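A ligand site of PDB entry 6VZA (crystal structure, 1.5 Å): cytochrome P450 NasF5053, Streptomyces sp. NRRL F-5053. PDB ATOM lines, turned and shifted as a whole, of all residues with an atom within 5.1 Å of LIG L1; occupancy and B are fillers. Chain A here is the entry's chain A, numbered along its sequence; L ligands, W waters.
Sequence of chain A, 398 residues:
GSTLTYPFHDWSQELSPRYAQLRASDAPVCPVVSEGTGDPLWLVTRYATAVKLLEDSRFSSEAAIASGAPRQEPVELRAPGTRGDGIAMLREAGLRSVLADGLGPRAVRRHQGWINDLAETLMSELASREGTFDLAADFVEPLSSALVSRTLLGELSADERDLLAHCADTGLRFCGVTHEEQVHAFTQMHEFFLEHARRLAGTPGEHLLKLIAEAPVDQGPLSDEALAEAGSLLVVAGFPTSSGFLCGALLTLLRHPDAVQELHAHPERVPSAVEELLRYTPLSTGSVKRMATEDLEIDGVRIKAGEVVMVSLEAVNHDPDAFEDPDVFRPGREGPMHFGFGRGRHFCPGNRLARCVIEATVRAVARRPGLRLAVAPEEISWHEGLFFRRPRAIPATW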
ATOM      1  N   GLN A  72       0.108 -12.713  22.224  1.00  0.00           N
ATOM      2  CA  GLN A  72       0.546 -11.560  21.462  1.00  0.00           C
ATOM      3  C   GLN A  72       1.806 -10.936  22.036  1.00  0.00           C
ATOM      4  O   GLN A  72       2.559 -10.301  21.276  1.00  0.00           O
ATOM      5  CB  GLN A  72      -0.595 -10.530  21.436  1.00  0.00           C
ATOM      6  CG  GLN A  72      -0.876  -9.897  22.776  1.00  0.00           C
ATOM      7  CD  GLN A  72      -2.222  -9.174  22.816  1.00  0.00           C
ATOM      8  OE1 GLN A  72      -2.345  -8.019  22.359  1.00  0.00           O
ATOM      9  NE2 GLN A  72      -3.199  -9.822  23.363  1.00  0.00           N
ATOM     10  N   GLU A  73       2.081 -11.114  23.316  1.00  0.00           N
ATOM     11  CA  GLU A  73       3.174 -10.435  24.021  1.00  0.00           C
ATOM     12  C   GLU A  73       4.444 -11.279  23.951  1.00  0.00           C
ATOM     13  O   GLU A  73       4.381 -12.515  23.892  1.00  0.00           O
ATOM     14  CB  GLU A  73       2.771 -10.201  25.492  1.00  0.00           C
ATOM     15  CG  GLU A  73       2.499 -11.443  26.344  1.00  0.00           C
ATOM     16  CD  GLU A  73       1.046 -11.923  26.368  1.00  0.00           C
ATOM     17  OE1 GLU A  73       0.306 -11.660  25.416  1.00  0.00           O
ATOM     18  OE2 GLU A  73       0.596 -12.602  27.341  1.00  0.00           O
ATOM     19  N   LEU A  77       3.631 -12.737  31.213  1.00  0.00           N
ATOM     20  CA  LEU A  77       3.397 -11.634  32.146  1.00  0.00           C
ATOM     21  C   LEU A  77       3.292 -12.132  33.586  1.00  0.00           C
ATOM     22  O   LEU A  77       2.274 -11.999  34.283  1.00  0.00           O
ATOM     23  CB  LEU A  77       2.141 -10.861  31.723  1.00  0.00           C
ATOM     24  CG  LEU A  77       2.107 -10.362  30.280  1.00  0.00           C
ATOM     25  CD1 LEU A  77       0.776  -9.679  30.016  1.00  0.00           C
ATOM     26  CD2 LEU A  77       3.252  -9.444  29.968  1.00  0.00           C
ATOM     27  N   PHE A 174       5.636  -4.530  24.185  1.00  0.00           N
ATOM     28  CA  PHE A 174       5.773  -5.379  23.013  1.00  0.00           C
ATOM     29  C   PHE A 174       7.187  -5.382  22.469  1.00  0.00           C
ATOM     30  O   PHE A 174       7.575  -6.359  21.808  1.00  0.00           O
ATOM     31  CB  PHE A 174       4.857  -4.875  21.908  1.00  0.00           C
ATOM     32  CG  PHE A 174       3.438  -5.279  22.078  1.00  0.00           C
ATOM     33  CD1 PHE A 174       3.058  -6.600  21.916  1.00  0.00           C
ATOM     34  CD2 PHE A 174       2.450  -4.336  22.361  1.00  0.00           C
ATOM     35  CE1 PHE A 174       1.755  -6.987  22.055  1.00  0.00           C
ATOM     36  CE2 PHE A 174       1.138  -4.729  22.469  1.00  0.00           C
ATOM     37  CZ  PHE A 174       0.788  -6.050  22.343  1.00  0.00           C
ATOM     38  N   THR A 241      -2.376   1.625  33.355  1.00  0.00           N
ATOM     39  CA  THR A 241      -3.652   1.860  32.709  1.00  0.00           C
ATOM     40  C   THR A 241      -4.177   3.242  33.086  1.00  0.00           C
ATOM     41  O   THR A 241      -4.469   4.053  32.201  1.00  0.00           O
ATOM     42  CB  THR A 241      -4.617   0.772  33.182  1.00  0.00           C
ATOM     43  OG1 THR A 241      -4.540   0.742  34.620  1.00  0.00           O
ATOM     44  CG2 THR A 241      -4.231  -0.566  32.612  1.00  0.00           C
ATOM     45  N   LEU A 283      -6.114   3.466  24.404  1.00  0.00           N
ATOM     46  CA  LEU A 283      -5.235   3.119  25.514  1.00  0.00           C
ATOM     47  C   LEU A 283      -4.326   1.954  25.129  1.00  0.00           C
ATOM     48  O   LEU A 283      -3.140   2.153  24.868  1.00  0.00           O
ATOM     49  CB  LEU A 283      -6.033   2.838  26.777  1.00  0.00           C
ATOM     50  CG  LEU A 283      -5.187   2.525  28.021  1.00  0.00           C
ATOM     51  CD1 LEU A 283      -4.210   3.630  28.317  1.00  0.00           C
ATOM     52  CD2 LEU A 283      -6.069   2.232  29.216  1.00  0.00           C
ATOM     53  N   SER A 284      -4.857   0.750  25.042  1.00  0.00           N
ATOM     54  CA  SER A 284      -3.992  -0.375  24.741  1.00  0.00           C
ATOM     55  C   SER A 284      -3.587  -0.400  23.284  1.00  0.00           C
ATOM     56  O   SER A 284      -4.380  -0.113  22.396  1.00  0.00           O
ATOM     57  CB  SER A 284      -4.710  -1.671  25.121  1.00  0.00           C
ATOM     58  OG  SER A 284      -3.910  -2.783  24.752  1.00  0.00           O
ATOM     59  N   THR A 285      -2.322  -0.772  23.044  1.00  0.00           N
ATOM     60  CA  THR A 285      -1.810  -1.037  21.713  1.00  0.00           C
ATOM     61  C   THR A 285      -1.932  -2.510  21.340  1.00  0.00           C
ATOM     62  O   THR A 285      -1.526  -2.912  20.239  1.00  0.00           O
ATOM     63  CB  THR A 285      -0.321  -0.640  21.673  1.00  0.00           C
ATOM     64  OG1 THR A 285       0.387  -1.459  22.608  1.00  0.00           O
ATOM     65  CG2 THR A 285      -0.137   0.804  22.030  1.00  0.00           C
ATOM     66  N   GLY A 286      -2.410  -3.325  22.272  1.00  0.00           N
ATOM     67  CA  GLY A 286      -2.756  -4.691  21.996  1.00  0.00           C
ATOM     68  C   GLY A 286      -4.238  -4.925  22.085  1.00  0.00           C
ATOM     69  O   GLY A 286      -5.055  -4.026  21.827  1.00  0.00           O
ATOM     70  N   SER A 287      -4.610  -6.159  22.404  1.00  0.00           N
ATOM     71  CA  SER A 287      -6.001  -6.561  22.363  1.00  0.00           C
ATOM     72  C   SER A 287      -6.379  -7.402  23.581  1.00  0.00           C
ATOM     73  O   SER A 287      -5.549  -8.133  24.143  1.00  0.00           O
ATOM     74  CB  SER A 287      -6.281  -7.445  21.146  1.00  0.00           C
ATOM     75  OG  SER A 287      -6.301  -6.702  19.954  1.00  0.00           O
ATOM     76  N   VAL A 288      -7.636  -7.303  23.982  1.00  0.00           N
ATOM     77  CA  VAL A 288      -8.155  -8.314  24.899  1.00  0.00           C
ATOM     78  C   VAL A 288      -8.152  -9.637  24.130  1.00  0.00           C
ATOM     79  O   VAL A 288      -8.233  -9.681  22.910  1.00  0.00           O
ATOM     80  CB  VAL A 288      -9.557  -8.010  25.425  1.00  0.00           C
ATOM     81  CG1 VAL A 288      -9.645  -6.698  26.118  1.00  0.00           C
ATOM     82  CG2 VAL A 288     -10.584  -8.132  24.330  1.00  0.00           C
ATOM     83  N   LYS A 289      -8.077 -10.740  24.869  1.00  0.00           N
ATOM     84  CA  LYS A 289      -7.965 -12.029  24.204  1.00  0.00           C
ATOM     85  C   LYS A 289      -8.580 -13.141  25.026  1.00  0.00           C
ATOM     86  O   LYS A 289      -8.677 -13.052  26.245  1.00  0.00           O
ATOM     87  CB  LYS A 289      -6.524 -12.320  23.785  1.00  0.00           C
ATOM     88  CG  LYS A 289      -5.644 -12.885  24.860  1.00  0.00           C
ATOM     89  CD  LYS A 289      -5.456 -11.946  25.978  1.00  0.00           C
ATOM     90  CE  LYS A 289      -4.328 -12.369  26.877  1.00  0.00           C
ATOM     91  NZ  LYS A 289      -4.387 -11.646  28.183  1.00  0.00           N
ATOM     92  N   LEU A 313     -10.010  -3.219  21.405  1.00  0.00           N
ATOM     93  CA  LEU A 313     -11.055  -2.322  21.919  1.00  0.00           C
ATOM     94  C   LEU A 313     -11.064  -0.999  21.183  1.00  0.00           C
ATOM     95  O   LEU A 313     -12.139  -0.400  20.981  1.00  0.00           O
ATOM     96  CB  LEU A 313     -10.862  -2.108  23.404  1.00  0.00           C
ATOM     97  CG  LEU A 313     -10.793  -3.363  24.270  1.00  0.00           C
ATOM     98  CD1 LEU A 313     -10.613  -3.007  25.743  1.00  0.00           C
ATOM     99  CD2 LEU A 313     -11.981  -4.250  24.071  1.00  0.00           C
ATOM    100  N   GLY A 340     -14.365   0.729  26.267  1.00  0.00           N
ATOM    101  CA  GLY A 340     -13.189   1.183  26.971  1.00  0.00           C
ATOM    102  C   GLY A 340     -12.830   0.363  28.200  1.00  0.00           C
ATOM    103  O   GLY A 340     -11.651   0.298  28.577  1.00  0.00           O
ATOM    104  N   PHE A 387       2.303  -1.553  26.211  1.00  0.00           N
ATOM    105  CA  PHE A 387       0.943  -2.043  26.051  1.00  0.00           C
ATOM    106  C   PHE A 387      -0.058  -0.899  26.206  1.00  0.00           C
ATOM    107  O   PHE A 387      -1.092  -0.874  25.540  1.00  0.00           O
ATOM    108  CB  PHE A 387       0.612  -3.079  27.124  1.00  0.00           C
ATOM    109  CG  PHE A 387       1.368  -4.381  27.039  1.00  0.00           C
ATOM    110  CD1 PHE A 387       2.108  -4.772  25.936  1.00  0.00           C
ATOM    111  CD2 PHE A 387       1.256  -5.255  28.108  1.00  0.00           C
ATOM    112  CE1 PHE A 387       2.769  -6.005  25.909  1.00  0.00           C
ATOM    113  CE2 PHE A 387       1.891  -6.481  28.098  1.00  0.00           C
ATOM    114  CZ  PHE A 387       2.644  -6.854  26.983  1.00  0.00           C
ATOM    115  N   PHE A 388       0.210   0.026  27.133  1.00  0.00           N
ATOM    116  CA  PHE A 388      -0.722   1.097  27.451  1.00  0.00           C
ATOM    117  C   PHE A 388      -0.073   2.425  27.099  1.00  0.00           C
ATOM    118  O   PHE A 388       0.887   2.844  27.749  1.00  0.00           O
ATOM    119  CB  PHE A 388      -1.129   0.986  28.933  1.00  0.00           C
ATOM    120  CG  PHE A 388      -1.688  -0.370  29.295  1.00  0.00           C
ATOM    121  CD1 PHE A 388      -2.864  -0.790  28.728  1.00  0.00           C
ATOM    122  CD2 PHE A 388      -0.992  -1.221  30.126  1.00  0.00           C
ATOM    123  CE1 PHE A 388      -3.373  -2.051  28.999  1.00  0.00           C
ATOM    124  CE2 PHE A 388      -1.511  -2.491  30.408  1.00  0.00           C
ATOM    125  CZ  PHE A 388      -2.681  -2.891  29.842  1.00  0.00           C
HETATM  126  C1  LIG L   1      -4.156  -7.743  27.444  1.00  0.00           C
HETATM  127  N1  LIG L   1      -4.038  -5.417  26.645  1.00  0.00           N
HETATM  128  O1  LIG L   1      -4.805  -8.737  27.640  1.00  0.00           O
HETATM  129  C2  LIG L   1      -4.620  -6.345  27.554  1.00  0.00           C
HETATM  130  C3  LIG L   1      -6.202  -6.310  27.324  1.00  0.00           C
HETATM  131  C4  LIG L   1      -6.609  -4.816  27.465  1.00  0.00           C
HETATM  132  O2  LIG L   1      -2.105  -4.675  25.624  1.00  0.00           O
HETATM  133  C5  LIG L   1      -0.735  -8.721  26.351  1.00  0.00           C
HETATM  134  C6  LIG L   1      -0.957  -7.258  25.806  1.00  0.00           C
HETATM  135  C7  LIG L   1      -1.981  -9.136  26.865  1.00  0.00           C
HETATM  136  C8  LIG L   1      -2.670  -5.480  26.308  1.00  0.00           C
HETATM  137  C9  LIG L   1      -1.980  -6.694  26.893  1.00  0.00           C
HETATM  138  N2  LIG L   1      -2.795  -7.813  27.087  1.00  0.00           N
HETATM  139  C10 LIG L   1      -7.020  -4.131  26.323  1.00  0.00           C
HETATM  140  C11 LIG L   1      -6.618  -3.926  28.494  1.00  0.00           C
HETATM  141  N3  LIG L   1      -7.265  -2.837  26.686  1.00  0.00           N
HETATM  142  C12 LIG L   1      -7.014  -2.685  28.039  1.00  0.00           C
HETATM  143  C13 LIG L   1      -6.280  -4.096  29.854  1.00  0.00           C
HETATM  144  C14 LIG L   1      -6.769  -1.750  30.243  1.00  0.00           C
HETATM  145  C15 LIG L   1      -7.089  -1.577  28.911  1.00  0.00           C
HETATM  146  C16 LIG L   1      -6.353  -2.997  30.704  1.00  0.00           C
HETATM  147  C1  LG2 L   2      -9.763  -5.432  33.314  1.00  0.00           C
HETATM  148  C2  LG2 L   2      -9.653  -1.042  31.281  1.00  0.00           C
HETATM  149  C3  LG2 L   2      -8.169   0.832  35.506  1.00  0.00           C
HETATM  150  C4  LG2 L   2      -8.383  -3.526  37.553  1.00  0.00           C
HETATM  151  C5  LG2 L   2      -9.878  -4.432  32.397  1.00  0.00           C
HETATM  152  C6  LG2 L   2     -10.308  -4.570  31.040  1.00  0.00           C
HETATM  153  C7  LG2 L   2     -10.247  -3.373  30.490  1.00  0.00           C
HETATM  154  C8  LG2 L   2      -9.806  -2.410  31.470  1.00  0.00           C
HETATM  155  C9  LG2 L   2     -10.596  -2.995  29.043  1.00  0.00           C
HETATM  156  C10 LG2 L   2     -10.793  -5.904  30.395  1.00  0.00           C
HETATM  157  C11 LG2 L   2      -9.701  -6.840  29.949  1.00  0.00           C
HETATM  158  C12 LG2 L   2     -10.265  -8.098  29.328  1.00  0.00           C
HETATM  159  O1  LG2 L   2      -9.494  -9.100  29.245  1.00  0.00           O
HETATM  160  O2  LG2 L   2     -11.439  -8.127  28.909  1.00  0.00           O
HETATM  161  C13 LG2 L   2      -9.226  -0.148  32.245  1.00  0.00           C
HETATM  162  C14 LG2 L   2      -9.052   1.256  32.056  1.00  0.00           C
HETATM  163  C15 LG2 L   2      -8.631   1.794  33.226  1.00  0.00           C
HETATM  164  C16 LG2 L   2      -8.515   0.710  34.164  1.00  0.00           C
HETATM  165  C17 LG2 L   2      -9.360   2.012  30.758  1.00  0.00           C
HETATM  166  C18 LG2 L   2      -8.327   3.279  33.493  1.00  0.00           C
HETATM  167  C19 LG2 L   2      -7.964   3.804  34.663  1.00  0.00           C
HETATM  168  C20 LG2 L   2      -8.148  -0.150  36.454  1.00  0.00           C
HETATM  169  C21 LG2 L   2      -7.855   0.027  37.863  1.00  0.00           C
HETATM  170  C22 LG2 L   2      -7.918  -1.200  38.399  1.00  0.00           C
HETATM  171  C23 LG2 L   2      -8.257  -2.161  37.390  1.00  0.00           C
HETATM  172  C24 LG2 L   2      -7.561   1.388  38.528  1.00  0.00           C
HETATM  173  C25 LG2 L   2      -7.711  -1.691  39.840  1.00  0.00           C
HETATM  174  C26 LG2 L   2      -7.616  -0.843  40.864  1.00  0.00           C
HETATM  175  C27 LG2 L   2      -8.653  -4.447  36.565  1.00  0.00           C
HETATM  176  C28 LG2 L   2      -8.630  -5.888  36.680  1.00  0.00           C
HETATM  177  C29 LG2 L   2      -8.999  -6.421  35.501  1.00  0.00           C
HETATM  178  C30 LG2 L   2      -9.285  -5.307  34.620  1.00  0.00           C
HETATM  179  C31 LG2 L   2      -8.186  -6.600  37.957  1.00  0.00           C
HETATM  180  C32 LG2 L   2      -9.106  -7.920  35.132  1.00  0.00           C
HETATM  181  C33 LG2 L   2     -10.550  -8.355  35.046  1.00  0.00           C
HETATM  182  C34 LG2 L   2     -10.689  -9.796  34.557  1.00  0.00           C
HETATM  183  O3  LG2 L   2     -11.750 -10.342  34.886  1.00  0.00           O
HETATM  184  O4  LG2 L   2      -9.770 -10.308  33.876  1.00  0.00           O
HETATM  185  N1  LG2 L   2      -9.576  -3.093  32.658  1.00  0.00           N
HETATM  186  N2  LG2 L   2      -8.867  -0.489  33.550  1.00  0.00           N
HETATM  187  N3  LG2 L   2      -8.457  -1.488  36.205  1.00  0.00           N
HETATM  188  N4  LG2 L   2      -9.062  -4.124  35.299  1.00  0.00           N
HETATM  189 FE1  LG2 L   2      -9.209  -2.238  34.480  1.00  0.00          FE
HETATM  190  C1  LG3 L   3      -4.861 -10.466  31.726  1.00  0.00           C
HETATM  191  N1  LG3 L   3      -6.761 -10.097  33.342  1.00  0.00           N
HETATM  192  O1  LG3 L   3      -4.364 -10.603  30.629  1.00  0.00           O
HETATM  193  C2  LG3 L   3      -6.282 -10.195  32.026  1.00  0.00           C
HETATM  194  C3  LG3 L   3      -6.495  -8.774  31.249  1.00  0.00           C
HETATM  195  C4  LG3 L   3      -5.609  -7.603  31.806  1.00  0.00           C
HETATM  196  O2  LG3 L   3      -6.304 -10.037  35.567  1.00  0.00           O
HETATM  197  C5  LG3 L   3      -2.127  -9.504  33.795  1.00  0.00           C
HETATM  198  C6  LG3 L   3      -3.458  -9.143  34.600  1.00  0.00           C
HETATM  199  C7  LG3 L   3      -2.417 -10.641  33.042  1.00  0.00           C
HETATM  200  C8  LG3 L   3      -5.902 -10.112  34.444  1.00  0.00           C
HETATM  201  C9  LG3 L   3      -4.422 -10.327  34.139  1.00  0.00           C
HETATM  202  N2  LG3 L   3      -3.976 -10.501  32.872  1.00  0.00           N
HETATM  203  C10 LG3 L   3      -6.222  -6.725  32.685  1.00  0.00           C
HETATM  204  C11 LG3 L   3      -4.331  -7.172  31.596  1.00  0.00           C
HETATM  205  N3  LG3 L   3      -5.306  -5.761  33.038  1.00  0.00           N
HETATM  206  C12 LG3 L   3      -4.123  -6.053  32.383  1.00  0.00           C
HETATM  207  C13 LG3 L   3      -3.253  -7.656  30.825  1.00  0.00           C
HETATM  208  C14 LG3 L   3      -1.851  -5.883  31.629  1.00  0.00           C
HETATM  209  C15 LG3 L   3      -2.893  -5.390  32.403  1.00  0.00           C
HETATM  210  C16 LG3 L   3      -2.038  -7.009  30.847  1.00  0.00           C
HETATM  211  O   HOH W   1      -7.650  -0.199  25.571  1.00  0.00           O
HETATM  212  O   HOH W   2      -6.578  -3.173  34.030  1.00  0.00           O
HETATM  213  O   HOH W   3      -7.417  -9.836  27.757  1.00  0.00           O
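O1 of LG3 L3 sits at hydrogen-bond distance from NZ of Lys 289 (2.7 Å).
O1 of LIG L1 is in hydrogen-bond range of NZ of Lys 289, at 3.0 Å.
The side-chain hydroxyl of Ser 284 is in hydrogen-bond range of an oxygen (O2) of LIG L1 (2.8 Å).
O4 of LG2 L2 lies within hydrogen-bond range of N1 of LG3 L3 (3.1 Å).
OG of Ser 284 lies close to O of Phe 387 (3.5 Å).
OG of Ser 284 lies within hydrogen-bond range of N of Gly 286.
N of Ser 287 sits at hydrogen-bond distance from OE1 of Gln 72 (2.9 Å).
O of Phe 387 lies within hydrogen-bond range of N of Thr 285, 2.8 Å away.
Merely in contact with LIG L1: Gln 72 (3.8 Å), Glu 73 (3.3 Å), Thr 241 (3.7 Å), Leu 283 (3.95 Å), Gly 286 (3.6 Å), Ser 287 (3.6 Å), Val 288 (3.7 Å), Leu 313 (3.5 Å), Phe 387 (3.5 Å) and Phe 388 (3.6 Å).
12 residues have an atom within 4 Å of LIG L1: Gln 72, Glu 73, Thr 241, Leu 283, Ser 284, Gly 286, Ser 287, Val 288, Lys 289, Leu 313, Phe 387 and Phe 388.
The nearest printed residue that does not touch LIG L1 is Phe 174 (4.1 Å).
Water W3 lies within hydrogen-bond range of an oxygen (O1) of LG2 L2 (2.7 Å), an oxygen (O1) of LIG L1 (2.8 Å) and the backbone NH (N) of Lys 289 (3.1 Å).
Water W1 bridges a nitrogen (N3) of LIG L1 (2.9 Å) and the backbone NH of Ser 284 (3.0 Å).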
